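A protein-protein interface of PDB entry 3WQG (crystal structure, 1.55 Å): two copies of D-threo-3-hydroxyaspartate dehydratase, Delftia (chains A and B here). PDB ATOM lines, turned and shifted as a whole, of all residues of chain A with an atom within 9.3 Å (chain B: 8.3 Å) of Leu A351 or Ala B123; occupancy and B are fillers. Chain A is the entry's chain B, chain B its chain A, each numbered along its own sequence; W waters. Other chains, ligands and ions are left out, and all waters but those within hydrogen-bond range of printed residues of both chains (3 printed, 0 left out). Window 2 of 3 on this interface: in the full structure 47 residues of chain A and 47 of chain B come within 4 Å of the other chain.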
ATOM      1  N   ALA A 272      10.418  21.467  -8.721  1.00  0.00           N
ATOM      2  CA  ALA A 272      11.767  21.236  -8.227  1.00  0.00           C
ATOM      3  C   ALA A 272      11.771  21.338  -6.748  1.00  0.00           C
ATOM      4  O   ALA A 272      10.929  22.038  -6.158  1.00  0.00           O
ATOM      5  CB  ALA A 272      12.764  22.288  -8.805  1.00  0.00           C
ATOM      6  N   THR A 273      12.782  20.712  -6.150  1.00  0.00           N
ATOM      7  CA  THR A 273      12.989  20.799  -4.680  1.00  0.00           C
ATOM      8  C   THR A 273      14.284  21.514  -4.352  1.00  0.00           C
ATOM      9  O   THR A 273      15.319  21.230  -4.972  1.00  0.00           O
ATOM     10  CB  THR A 273      12.998  19.344  -4.032  1.00  0.00           C
ATOM     11  OG1 THR A 273      11.751  18.671  -4.284  1.00  0.00           O
ATOM     12  CG2 THR A 273      13.268  19.406  -2.544  1.00  0.00           C
ATOM     13  N   VAL A 274      14.259  22.361  -3.279  1.00  0.00           N
ATOM     14  CA  VAL A 274      15.488  22.955  -2.790  1.00  0.00           C
ATOM     15  C   VAL A 274      16.300  21.893  -2.002  1.00  0.00           C
ATOM     16  O   VAL A 274      15.733  21.233  -1.071  1.00  0.00           O
ATOM     17  CB  VAL A 274      15.155  24.141  -1.858  1.00  0.00           C
ATOM     18  CG1 VAL A 274      16.460  24.678  -1.292  1.00  0.00           C
ATOM     19  CG2 VAL A 274      14.439  25.239  -2.685  1.00  0.00           C
ATOM     20  N   ILE A 275      17.554  21.654  -2.402  1.00  0.00           N
ATOM     21  CA  ILE A 275      18.375  20.594  -1.807  1.00  0.00           C
ATOM     22  C   ILE A 275      19.623  21.157  -1.096  1.00  0.00           C
ATOM     23  O   ILE A 275      20.441  20.417  -0.540  1.00  0.00           O
ATOM     24  CB  ILE A 275      18.816  19.525  -2.890  1.00  0.00           C
ATOM     25  CG1 ILE A 275      19.662  20.164  -4.032  1.00  0.00           C
ATOM     26  CG2 ILE A 275      17.587  18.771  -3.378  1.00  0.00           C
ATOM     27  CD1 ILE A 275      20.174  19.131  -5.020  1.00  0.00           C
ATOM     28  N   GLY A 276      19.788  22.472  -1.106  1.00  0.00           N
ATOM     29  CA  GLY A 276      21.007  23.038  -0.515  1.00  0.00           C
ATOM     30  C   GLY A 276      21.065  24.527  -0.704  1.00  0.00           C
ATOM     31  O   GLY A 276      20.155  25.109  -1.305  1.00  0.00           O
ATOM     32  N   HIS A 277      22.098  25.126  -0.120  1.00  0.00           N
ATOM     33  CA  HIS A 277      22.343  26.567  -0.227  1.00  0.00           C
ATOM     34  C   HIS A 277      23.823  26.877  -0.301  1.00  0.00           C
ATOM     35  O   HIS A 277      24.673  26.079   0.114  1.00  0.00           O
ATOM     36  CB  HIS A 277      21.740  27.312   0.986  1.00  0.00           C
ATOM     37  CG  HIS A 277      20.279  27.119   1.141  1.00  0.00           C
ATOM     38  ND1 HIS A 277      19.709  26.126   1.953  1.00  0.00           N
ATOM     39  CD2 HIS A 277      19.227  27.803   0.564  1.00  0.00           C
ATOM     40  CE1 HIS A 277      18.355  26.209   1.859  1.00  0.00           C
ATOM     41  NE2 HIS A 277      18.062  27.210   0.977  1.00  0.00           N
ATOM     42  N   ALA A 284      20.282  29.389  -3.636  1.00  0.00           N
ATOM     43  CA  ALA A 284      19.575  28.158  -3.228  1.00  0.00           C
ATOM     44  C   ALA A 284      19.913  27.120  -4.299  1.00  0.00           C
ATOM     45  O   ALA A 284      20.021  27.457  -5.471  1.00  0.00           O
ATOM     46  CB  ALA A 284      18.082  28.384  -3.147  1.00  0.00           C
ATOM     47  N   ILE A 285      20.121  25.858  -3.948  1.00  0.00           N
ATOM     48  CA  ILE A 285      20.476  24.812  -4.969  1.00  0.00           C
ATOM     49  C   ILE A 285      19.213  23.975  -5.103  1.00  0.00           C
ATOM     50  O   ILE A 285      18.667  23.539  -4.061  1.00  0.00           O
ATOM     51  CB  ILE A 285      21.667  23.899  -4.522  1.00  0.00           C
ATOM     52  CG1 ILE A 285      22.869  24.726  -4.003  1.00  0.00           C
ATOM     53  CG2 ILE A 285      22.031  22.871  -5.614  1.00  0.00           C
ATOM     54  CD1 ILE A 285      23.492  25.565  -5.037  1.00  0.00           C
ATOM     55  N   VAL A 286      18.747  23.727  -6.357  1.00  0.00           N
ATOM     56  CA  VAL A 286      17.540  22.941  -6.575  1.00  0.00           C
ATOM     57  C   VAL A 286      17.955  21.696  -7.392  1.00  0.00           C
ATOM     58  O   VAL A 286      19.038  21.657  -8.000  1.00  0.00           O
ATOM     59  CB  VAL A 286      16.429  23.715  -7.324  1.00  0.00           C
ATOM     60  CG1 VAL A 286      15.956  24.845  -6.396  1.00  0.00           C
ATOM     61  CG2 VAL A 286      16.860  24.244  -8.706  1.00  0.00           C
ATOM     62  N   ILE A 345      19.055  33.605   2.262  1.00  0.00           N
ATOM     63  CA  ILE A 345      18.485  32.763   1.194  1.00  0.00           C
ATOM     64  C   ILE A 345      17.868  31.474   1.727  1.00  0.00           C
ATOM     65  O   ILE A 345      16.858  31.019   1.187  1.00  0.00           O
ATOM     66  CB  ILE A 345      19.485  32.468   0.054  1.00  0.00           C
ATOM     67  CG1 ILE A 345      18.739  31.834  -1.155  1.00  0.00           C
ATOM     68  CG2 ILE A 345      20.645  31.611   0.538  1.00  0.00           C
ATOM     69  CD1 ILE A 345      18.119  32.814  -2.153  1.00  0.00           C
ATOM     70  N   ALA A 346      18.403  30.959   2.858  1.00  0.00           N
ATOM     71  CA  ALA A 346      17.877  29.701   3.455  1.00  0.00           C
ATOM     72  C   ALA A 346      16.503  29.940   4.066  1.00  0.00           C
ATOM     73  O   ALA A 346      15.698  29.019   4.166  1.00  0.00           O
ATOM     74  CB  ALA A 346      18.836  29.121   4.502  1.00  0.00           C
ATOM     75  N   THR A 347      16.231  31.161   4.536  1.00  0.00           N
ATOM     76  CA  THR A 347      14.898  31.383   5.104  1.00  0.00           C
ATOM     77  C   THR A 347      13.927  31.733   3.935  1.00  0.00           C
ATOM     78  O   THR A 347      12.779  31.341   3.926  1.00  0.00           O
ATOM     79  CB  THR A 347      14.856  32.265   6.432  1.00  0.00           C
ATOM     80  OG1 THR A 347      14.580  33.594   6.086  1.00  0.00           O
ATOM     81  CG2 THR A 347      16.155  32.160   7.327  1.00  0.00           C
ATOM     82  N   ARG A 348      14.421  32.408   2.898  1.00  0.00           N
ATOM     83  CA  ARG A 348      13.588  32.646   1.713  1.00  0.00           C
ATOM     84  C   ARG A 348      13.169  31.340   0.989  1.00  0.00           C
ATOM     85  O   ARG A 348      12.046  31.201   0.465  1.00  0.00           O
ATOM     86  CB  ARG A 348      14.351  33.478   0.713  1.00  0.00           C
ATOM     87  CG  ARG A 348      13.426  34.232  -0.193  1.00  0.00           C
ATOM     88  CD  ARG A 348      12.739  35.309   0.617  1.00  0.00           C
ATOM     89  NE  ARG A 348      12.653  36.515  -0.180  1.00  0.00           N
ATOM     90  CZ  ARG A 348      11.716  36.749  -1.089  1.00  0.00           C
ATOM     91  NH1 ARG A 348      10.744  35.867  -1.302  1.00  0.00           N
ATOM     92  NH2 ARG A 348      11.747  37.890  -1.757  1.00  0.00           N
ATOM     93  N   PHE A 349      14.097  30.411   0.962  1.00  0.00           N
ATOM     94  CA  PHE A 349      13.915  29.127   0.269  1.00  0.00           C
ATOM     95  C   PHE A 349      14.363  27.939   1.126  1.00  0.00           C
ATOM     96  O   PHE A 349      15.460  27.406   0.904  1.00  0.00           O
ATOM     97  CB  PHE A 349      14.655  29.131  -1.095  1.00  0.00           C
ATOM     98  CG  PHE A 349      14.070  30.102  -2.088  1.00  0.00           C
ATOM     99  CD1 PHE A 349      12.853  29.807  -2.785  1.00  0.00           C
ATOM    100  CD2 PHE A 349      14.698  31.382  -2.313  1.00  0.00           C
ATOM    101  CE1 PHE A 349      12.336  30.768  -3.716  1.00  0.00           C
ATOM    102  CE2 PHE A 349      14.160  32.315  -3.215  1.00  0.00           C
ATOM    103  CZ  PHE A 349      12.980  32.018  -3.916  1.00  0.00           C
ATOM    104  N   PRO A 350      13.522  27.518   2.093  1.00  0.00           N
ATOM    105  CA  PRO A 350      14.052  26.502   3.026  1.00  0.00           C
ATOM    106  C   PRO A 350      14.329  25.132   2.353  1.00  0.00           C
ATOM    107  O   PRO A 350      13.661  24.795   1.359  1.00  0.00           O
ATOM    108  CB  PRO A 350      12.943  26.384   4.115  1.00  0.00           C
ATOM    109  CG  PRO A 350      12.134  27.670   3.986  1.00  0.00           C
ATOM    110  CD  PRO A 350      12.203  28.043   2.508  1.00  0.00           C
ATOM    111  N   LEU A 351      15.303  24.379   2.892  1.00  0.00           N
ATOM    112  CA  LEU A 351      15.591  23.047   2.427  1.00  0.00           C
ATOM    113  C   LEU A 351      14.264  22.299   2.315  1.00  0.00           C
ATOM    114  O   LEU A 351      13.399  22.448   3.203  1.00  0.00           O
ATOM    115  CB  LEU A 351      16.640  22.350   3.360  1.00  0.00           C
ATOM    116  CG  LEU A 351      16.880  20.822   3.139  1.00  0.00           C
ATOM    117  CD1 LEU A 351      17.788  20.424   1.942  1.00  0.00           C
ATOM    118  CD2 LEU A 351      17.254  20.054   4.438  1.00  0.00           C
ATOM    119  N   GLY A 352      14.051  21.567   1.202  1.00  0.00           N
ATOM    120  CA  GLY A 352      12.831  20.782   1.006  1.00  0.00           C
ATOM    121  C   GLY A 352      11.657  21.570   0.390  1.00  0.00           C
ATOM    122  O   GLY A 352      10.692  20.986  -0.021  1.00  0.00           O
ATOM    123  N   THR A 353      11.717  22.902   0.339  1.00  0.00           N
ATOM    124  CA  THR A 353      10.707  23.728  -0.374  1.00  0.00           C
ATOM    125  C   THR A 353      10.566  23.288  -1.815  1.00  0.00           C
ATOM    126  O   THR A 353      11.607  23.023  -2.501  1.00  0.00           O
ATOM    127  CB  THR A 353      11.133  25.220  -0.463  1.00  0.00           C
ATOM    128  OG1 THR A 353      11.407  25.702   0.840  1.00  0.00           O
ATOM    129  CG2 THR A 353      10.051  26.099  -1.165  1.00  0.00           C
ATOM    130  N   ARG A 354       9.315  23.247  -2.293  1.00  0.00           N
ATOM    131  CA  ARG A 354       9.076  22.897  -3.728  1.00  0.00           C
ATOM    132  C   ARG A 354       8.727  24.197  -4.441  1.00  0.00           C
ATOM    133  O   ARG A 354       7.914  25.049  -3.941  1.00  0.00           O
ATOM    134  CB  ARG A 354       7.885  21.935  -3.863  1.00  0.00           C
ATOM    135  CG  ARG A 354       8.261  20.529  -3.457  1.00  0.00           C
ATOM    136  CD  ARG A 354       7.101  19.553  -3.379  1.00  0.00           C
ATOM    137  NE  ARG A 354       7.796  18.290  -3.107  1.00  0.00           N
ATOM    138  CZ  ARG A 354       7.657  17.154  -3.765  1.00  0.00           C
ATOM    139  NH1 ARG A 354       6.693  16.996  -4.665  1.00  0.00           N
ATOM    140  NH2 ARG A 354       8.459  16.127  -3.413  1.00  0.00           N
ATOM    141  N   LEU A 355       9.261  24.302  -5.654  1.00  0.00           N
ATOM    142  CA  LEU A 355       9.145  25.480  -6.543  1.00  0.00           C
ATOM    143  C   LEU A 355       8.789  25.017  -7.922  1.00  0.00           C
ATOM    144  O   LEU A 355       8.841  23.846  -8.198  1.00  0.00           O
ATOM    145  CB  LEU A 355      10.493  26.217  -6.618  1.00  0.00           C
ATOM    146  CG  LEU A 355      10.996  26.745  -5.305  1.00  0.00           C
ATOM    147  CD1 LEU A 355      12.448  27.139  -5.450  1.00  0.00           C
ATOM    148  CD2 LEU A 355      10.128  27.861  -4.720  1.00  0.00           C
ATOM    149  N   SER B  96      23.443  16.361  -3.448  1.00  0.00           N
ATOM    150  CA  SER B  96      22.983  16.616  -2.087  1.00  0.00           C
ATOM    151  C   SER B  96      21.660  15.922  -1.870  1.00  0.00           C
ATOM    152  O   SER B  96      20.686  16.165  -2.602  1.00  0.00           O
ATOM    153  CB  SER B  96      22.756  18.107  -1.825  1.00  0.00           C
ATOM    154  OG  SER B  96      23.941  18.787  -2.083  1.00  0.00           O
ATOM    155  N   MET B  97      21.582  15.082  -0.827  1.00  0.00           N
ATOM    156  CA  MET B  97      20.397  14.269  -0.629  1.00  0.00           C
ATOM    157  C   MET B  97      19.166  15.093  -0.221  1.00  0.00           C
ATOM    158  O   MET B  97      19.226  15.917   0.739  1.00  0.00           O
ATOM    159  CB  MET B  97      20.734  13.231   0.477  1.00  0.00           C
ATOM    160  CG  MET B  97      19.506  12.310   0.711  1.00  0.00           C
ATOM    161  SD  MET B  97      19.120  11.344  -0.793  1.00  0.00           S
ATOM    162  CE  MET B  97      17.715  10.390  -0.124  1.00  0.00           C
ATOM    163  N   ALA B  98      18.058  14.915  -0.952  1.00  0.00           N
ATOM    164  CA  ALA B  98      16.735  15.431  -0.584  1.00  0.00           C
ATOM    165  C   ALA B  98      16.006  14.507   0.395  1.00  0.00           C
ATOM    166  O   ALA B  98      15.849  13.325   0.111  1.00  0.00           O
ATOM    167  CB  ALA B  98      15.853  15.620  -1.803  1.00  0.00           C
ATOM    168  N   PRO B  99      15.621  15.050   1.571  1.00  0.00           N
ATOM    169  CA  PRO B  99      14.973  14.132   2.522  1.00  0.00           C
ATOM    170  C   PRO B  99      13.755  13.417   1.950  1.00  0.00           C
ATOM    171  O   PRO B  99      13.527  12.275   2.358  1.00  0.00           O
ATOM    172  CB  PRO B  99      14.661  15.051   3.727  1.00  0.00           C
ATOM    173  CG  PRO B  99      15.776  16.072   3.697  1.00  0.00           C
ATOM    174  CD  PRO B  99      15.991  16.349   2.207  1.00  0.00           C
ATOM    175  N   HIS B 100      12.987  14.009   1.035  1.00  0.00           N
ATOM    176  CA  HIS B 100      11.797  13.326   0.539  1.00  0.00           C
ATOM    177  C   HIS B 100      12.151  12.042  -0.244  1.00  0.00           C
ATOM    178  O   HIS B 100      11.305  11.175  -0.425  1.00  0.00           O
ATOM    179  CB  HIS B 100      10.872  14.251  -0.250  1.00  0.00           C
ATOM    180  CG  HIS B 100      11.338  14.530  -1.635  1.00  0.00           C
ATOM    181  ND1 HIS B 100      12.134  15.594  -1.951  1.00  0.00           N
ATOM    182  CD2 HIS B 100      11.165  13.792  -2.812  1.00  0.00           C
ATOM    183  CE1 HIS B 100      12.418  15.534  -3.297  1.00  0.00           C
ATOM    184  NE2 HIS B 100      11.816  14.443  -3.809  1.00  0.00           N
ATOM    185  N   LEU B 102      14.280   9.905   0.866  1.00  0.00           N
ATOM    186  CA  LEU B 102      14.807   8.871   1.801  1.00  0.00           C
ATOM    187  C   LEU B 102      14.100   7.500   1.701  1.00  0.00           C
ATOM    188  O   LEU B 102      14.784   6.486   1.807  1.00  0.00           O
ATOM    189  CB  LEU B 102      14.805   9.428   3.238  1.00  0.00           C
ATOM    190  CG  LEU B 102      16.063  10.270   3.528  1.00  0.00           C
ATOM    191  CD1 LEU B 102      15.845  11.156   4.796  1.00  0.00           C
ATOM    192  CD2 LEU B 102      17.312   9.419   3.605  1.00  0.00           C
ATOM    193  N   VAL B 119      25.784  14.813   1.812  1.00  0.00           N
ATOM    194  CA  VAL B 119      25.102  16.030   2.362  1.00  0.00           C
ATOM    195  C   VAL B 119      26.171  17.111   2.608  1.00  0.00           C
ATOM    196  O   VAL B 119      27.382  16.820   2.634  1.00  0.00           O
ATOM    197  CB  VAL B 119      24.402  15.775   3.744  1.00  0.00           C
ATOM    198  CG1 VAL B 119      23.298  14.701   3.638  1.00  0.00           C
ATOM    199  CG2 VAL B 119      25.447  15.381   4.841  1.00  0.00           C
ATOM    200  N   ASP B 120      25.687  18.354   2.733  1.00  0.00           N
ATOM    201  CA  ASP B 120      26.591  19.477   3.045  1.00  0.00           C
ATOM    202  C   ASP B 120      25.920  20.421   4.050  1.00  0.00           C
ATOM    203  O   ASP B 120      26.336  21.558   4.213  1.00  0.00           O
ATOM    204  CB  ASP B 120      26.982  20.250   1.788  1.00  0.00           C
ATOM    205  CG  ASP B 120      25.780  20.977   1.122  1.00  0.00           C
ATOM    206  OD1 ASP B 120      24.602  20.926   1.574  1.00  0.00           O
ATOM    207  OD2 ASP B 120      26.020  21.682   0.148  1.00  0.00           O
ATOM    208  N   SER B 121      24.895  19.941   4.769  1.00  0.00           N
ATOM    209  CA  SER B 121      24.260  20.774   5.779  1.00  0.00           C
ATOM    210  C   SER B 121      23.912  19.962   6.993  1.00  0.00           C
ATOM    211  O   SER B 121      23.675  18.718   6.911  1.00  0.00           O
ATOM    212  CB  SER B 121      22.948  21.411   5.229  1.00  0.00           C
ATOM    213  OG  SER B 121      22.016  20.398   4.952  1.00  0.00           O
ATOM    214  N   VAL B 122      23.810  20.637   8.133  1.00  0.00           N
ATOM    215  CA  VAL B 122      23.344  19.949   9.334  1.00  0.00           C
ATOM    216  C   VAL B 122      21.894  19.484   9.202  1.00  0.00           C
ATOM    217  O   VAL B 122      21.607  18.345   9.620  1.00  0.00           O
ATOM    218  CB  VAL B 122      23.515  20.875  10.608  1.00  0.00           C
ATOM    219  CG1 VAL B 122      22.834  20.267  11.848  1.00  0.00           C
ATOM    220  CG2 VAL B 122      24.990  21.174  10.858  1.00  0.00           C
ATOM    221  N   ALA B 123      20.990  20.322   8.678  1.00  0.00           N
ATOM    222  CA  ALA B 123      19.568  19.914   8.464  1.00  0.00           C
ATOM    223  C   ALA B 123      19.405  18.632   7.633  1.00  0.00           C
ATOM    224  O   ALA B 123      18.584  17.768   7.995  1.00  0.00           O
ATOM    225  CB  ALA B 123      18.745  21.020   7.844  1.00  0.00           C
ATOM    226  N   ALA B 124      20.094  18.498   6.509  1.00  0.00           N
ATOM    227  CA  ALA B 124      19.991  17.247   5.759  1.00  0.00           C
ATOM    228  C   ALA B 124      20.609  16.069   6.539  1.00  0.00           C
ATOM    229  O   ALA B 124      20.060  14.977   6.476  1.00  0.00           O
ATOM    230  CB  ALA B 124      20.630  17.360   4.387  1.00  0.00           C
ATOM    231  N   ALA B 125      21.739  16.275   7.218  1.00  0.00           N
ATOM    232  CA  ALA B 125      22.318  15.200   8.028  1.00  0.00           C
ATOM    233  C   ALA B 125      21.312  14.762   9.139  1.00  0.00           C
ATOM    234  O   ALA B 125      21.133  13.507   9.372  1.00  0.00           O
ATOM    235  CB  ALA B 125      23.635  15.647   8.638  1.00  0.00           C
ATOM    236  N   GLN B 126      20.623  15.734   9.778  1.00  0.00           N
ATOM    237  CA  GLN B 126      19.657  15.385  10.825  1.00  0.00           C
ATOM    238  C   GLN B 126      18.502  14.591  10.217  1.00  0.00           C
ATOM    239  O   GLN B 126      18.013  13.621  10.852  1.00  0.00           O
ATOM    240  CB  GLN B 126      19.106  16.663  11.486  1.00  0.00           C
ATOM    241  CG  GLN B 126      20.131  17.375  12.363  1.00  0.00           C
ATOM    242  CD  GLN B 126      19.653  18.728  12.915  1.00  0.00           C
ATOM    243  OE1 GLN B 126      18.941  19.489  12.236  1.00  0.00           O
ATOM    244  NE2 GLN B 126      20.074  19.047  14.142  1.00  0.00           N
ATOM    245  N   ALA B 127      18.065  14.958   8.986  1.00  0.00           N
ATOM    246  CA  ALA B 127      16.870  14.319   8.421  1.00  0.00           C
ATOM    247  C   ALA B 127      17.259  12.849   8.135  1.00  0.00           C
ATOM    248  O   ALA B 127      16.507  11.917   8.425  1.00  0.00           O
ATOM    249  CB  ALA B 127      16.410  15.006   7.126  1.00  0.00           C
ATOM    250  N   ILE B 128      18.423  12.635   7.544  1.00  0.00           N
ATOM    251  CA  ILE B 128      18.889  11.229   7.318  1.00  0.00           C
ATOM    252  C   ILE B 128      19.013  10.434   8.596  1.00  0.00           C
ATOM    253  O   ILE B 128      18.470   9.277   8.700  1.00  0.00           O
ATOM    254  CB  ILE B 128      20.251  11.218   6.584  1.00  0.00           C
ATOM    255  CG1 ILE B 128      20.057  11.889   5.211  1.00  0.00           C
ATOM    256  CG2 ILE B 128      20.747   9.762   6.402  1.00  0.00           C
ATOM    257  CD1 ILE B 128      21.351  11.977   4.383  1.00  0.00           C
ATOM    258  N   ALA B 129      19.657  11.039   9.613  1.00  0.00           N
ATOM    259  CA  ALA B 129      19.986  10.242  10.817  1.00  0.00           C
ATOM    260  C   ALA B 129      18.697   9.918  11.564  1.00  0.00           C
ATOM    261  O   ALA B 129      18.500   8.756  12.049  1.00  0.00           O
ATOM    262  CB  ALA B 129      20.974  10.982  11.677  1.00  0.00           C
ATOM    263  N   ALA B 130      17.770  10.863  11.620  1.00  0.00           N
ATOM    264  CA  ALA B 130      16.486  10.590  12.298  1.00  0.00           C
ATOM    265  C   ALA B 130      15.661   9.483  11.592  1.00  0.00           C
ATOM    266  O   ALA B 130      15.167   8.512  12.221  1.00  0.00           O
ATOM    267  CB  ALA B 130      15.647  11.878  12.436  1.00  0.00           C
ATOM    268  N   LEU B 161      31.268  23.966  10.550  1.00  0.00           N
ATOM    269  CA  LEU B 161      30.177  23.301   9.817  1.00  0.00           C
ATOM    270  C   LEU B 161      30.527  21.828   9.508  1.00  0.00           C
ATOM    271  O   LEU B 161      29.679  20.941   9.717  1.00  0.00           O
ATOM    272  CB  LEU B 161      29.732  24.078   8.561  1.00  0.00           C
ATOM    273  CG  LEU B 161      28.705  23.461   7.615  1.00  0.00           C
ATOM    274  CD1 LEU B 161      27.336  23.240   8.292  1.00  0.00           C
ATOM    275  CD2 LEU B 161      28.604  24.249   6.317  1.00  0.00           C
ATOM    276  N   ALA B 164      30.175  19.814  12.741  1.00  0.00           N
ATOM    277  CA  ALA B 164      28.769  19.747  13.163  1.00  0.00           C
ATOM    278  C   ALA B 164      28.038  18.717  12.332  1.00  0.00           C
ATOM    279  O   ALA B 164      27.207  17.978  12.876  1.00  0.00           O
ATOM    280  CB  ALA B 164      28.076  21.096  13.035  1.00  0.00           C
ATOM    281  N   ILE B 165      28.310  18.665  11.016  1.00  0.00           N
ATOM    282  CA  ILE B 165      27.664  17.647  10.173  1.00  0.00           C
ATOM    283  C   ILE B 165      28.226  16.271  10.559  1.00  0.00           C
ATOM    284  O   ILE B 165      27.438  15.292  10.704  1.00  0.00           O
ATOM    285  CB  ILE B 165      27.922  17.939   8.663  1.00  0.00           C
ATOM    286  CG1 ILE B 165      27.340  19.308   8.306  1.00  0.00           C
ATOM    287  CG2 ILE B 165      27.395  16.793   7.717  1.00  0.00           C
ATOM    288  CD1 ILE B 165      27.818  19.818   6.955  1.00  0.00           C
ATOM    289  N   THR B 168      26.731  15.127  13.710  1.00  0.00           N
ATOM    290  CA  THR B 168      25.318  14.811  13.553  1.00  0.00           C
ATOM    291  C   THR B 168      25.203  13.364  12.983  1.00  0.00           C
ATOM    292  O   THR B 168      24.389  12.555  13.435  1.00  0.00           O
ATOM    293  CB  THR B 168      24.615  15.798  12.606  1.00  0.00           C
ATOM    294  OG1 THR B 168      24.583  17.059  13.231  1.00  0.00           O
ATOM    295  CG2 THR B 168      23.131  15.419  12.418  1.00  0.00           C
HETATM  296  O   HOH W   1      23.373  23.439   2.012  1.00  0.00           O
HETATM  297  O   HOH W   2      20.661  18.194   1.058  1.00  0.00           O
HETATM  298  O   HOH W   3      25.018  23.456  -1.141  1.00  0.00           O
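The side-chain hydroxyl (OG) of Ser B121 sits at hydrogen-bond distance from the backbone NH (N) of Ala B124 (3.1 Å). The backbone NH (N) of Ile A275 is in hydrogen-bond range of the backbone carbonyl oxygen (O) of Ile A285, 2.7 Å away.
Among the printed residues, merely in contact across the chains: Thr A273 with His B100, Ile A275 with Ser B96, Ile A275 with Ala B98, Leu A351 with Ala B123, Leu A351 with Ala B124 and Arg A354 with His B100.
Leu A351 touches two residues of chain B. Ala B123 touches one residue of chain A. Ala B124 touches just one residue of chain A: Leu A351 (3.8 Å). Printed residues of chain B within 4 Å of Arg A354: His B100 (3.6 Å). Of the printed residues of chain A, Ala B98 touches Ile A275 (3.9 Å). The nearest residue of chain B that does not touch Leu A351 is Pro B99 (4.3 Å). The nearest printed residue of chain B that does not touch Ile A275 is Asp B120 (4.7 Å).
Hydrophobic or aromatic side chains of chain B that line the printed part of chain A: Ala B98, His B100 and Ala B123. Of the 20 printed residues of chain A, 4 touch a printed residue of chain B. Along chain A the printed residues that touch a printed residue of chain B span positions 273 to 354. Among the printed residues, no Asp or Glu carboxylate lies within 4 Å of a Lys or Arg side-chain nitrogen of the other chain.
No position is printed for both chains.
Water W3 lies within hydrogen-bond range of OD2 of Asp B120 (2.4 Å) and O of His A277 (2.9 Å). Water W2 lies within hydrogen-bond range of the backbone carbonyl oxygen (O) of Met B97 and the backbone carbonyl oxygen (O) of Ile A275. Water W1 bridges the side-chain carboxylate of Asp B120 (2.8 Å) and the backbone NH of His A277 (3.0 Å).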
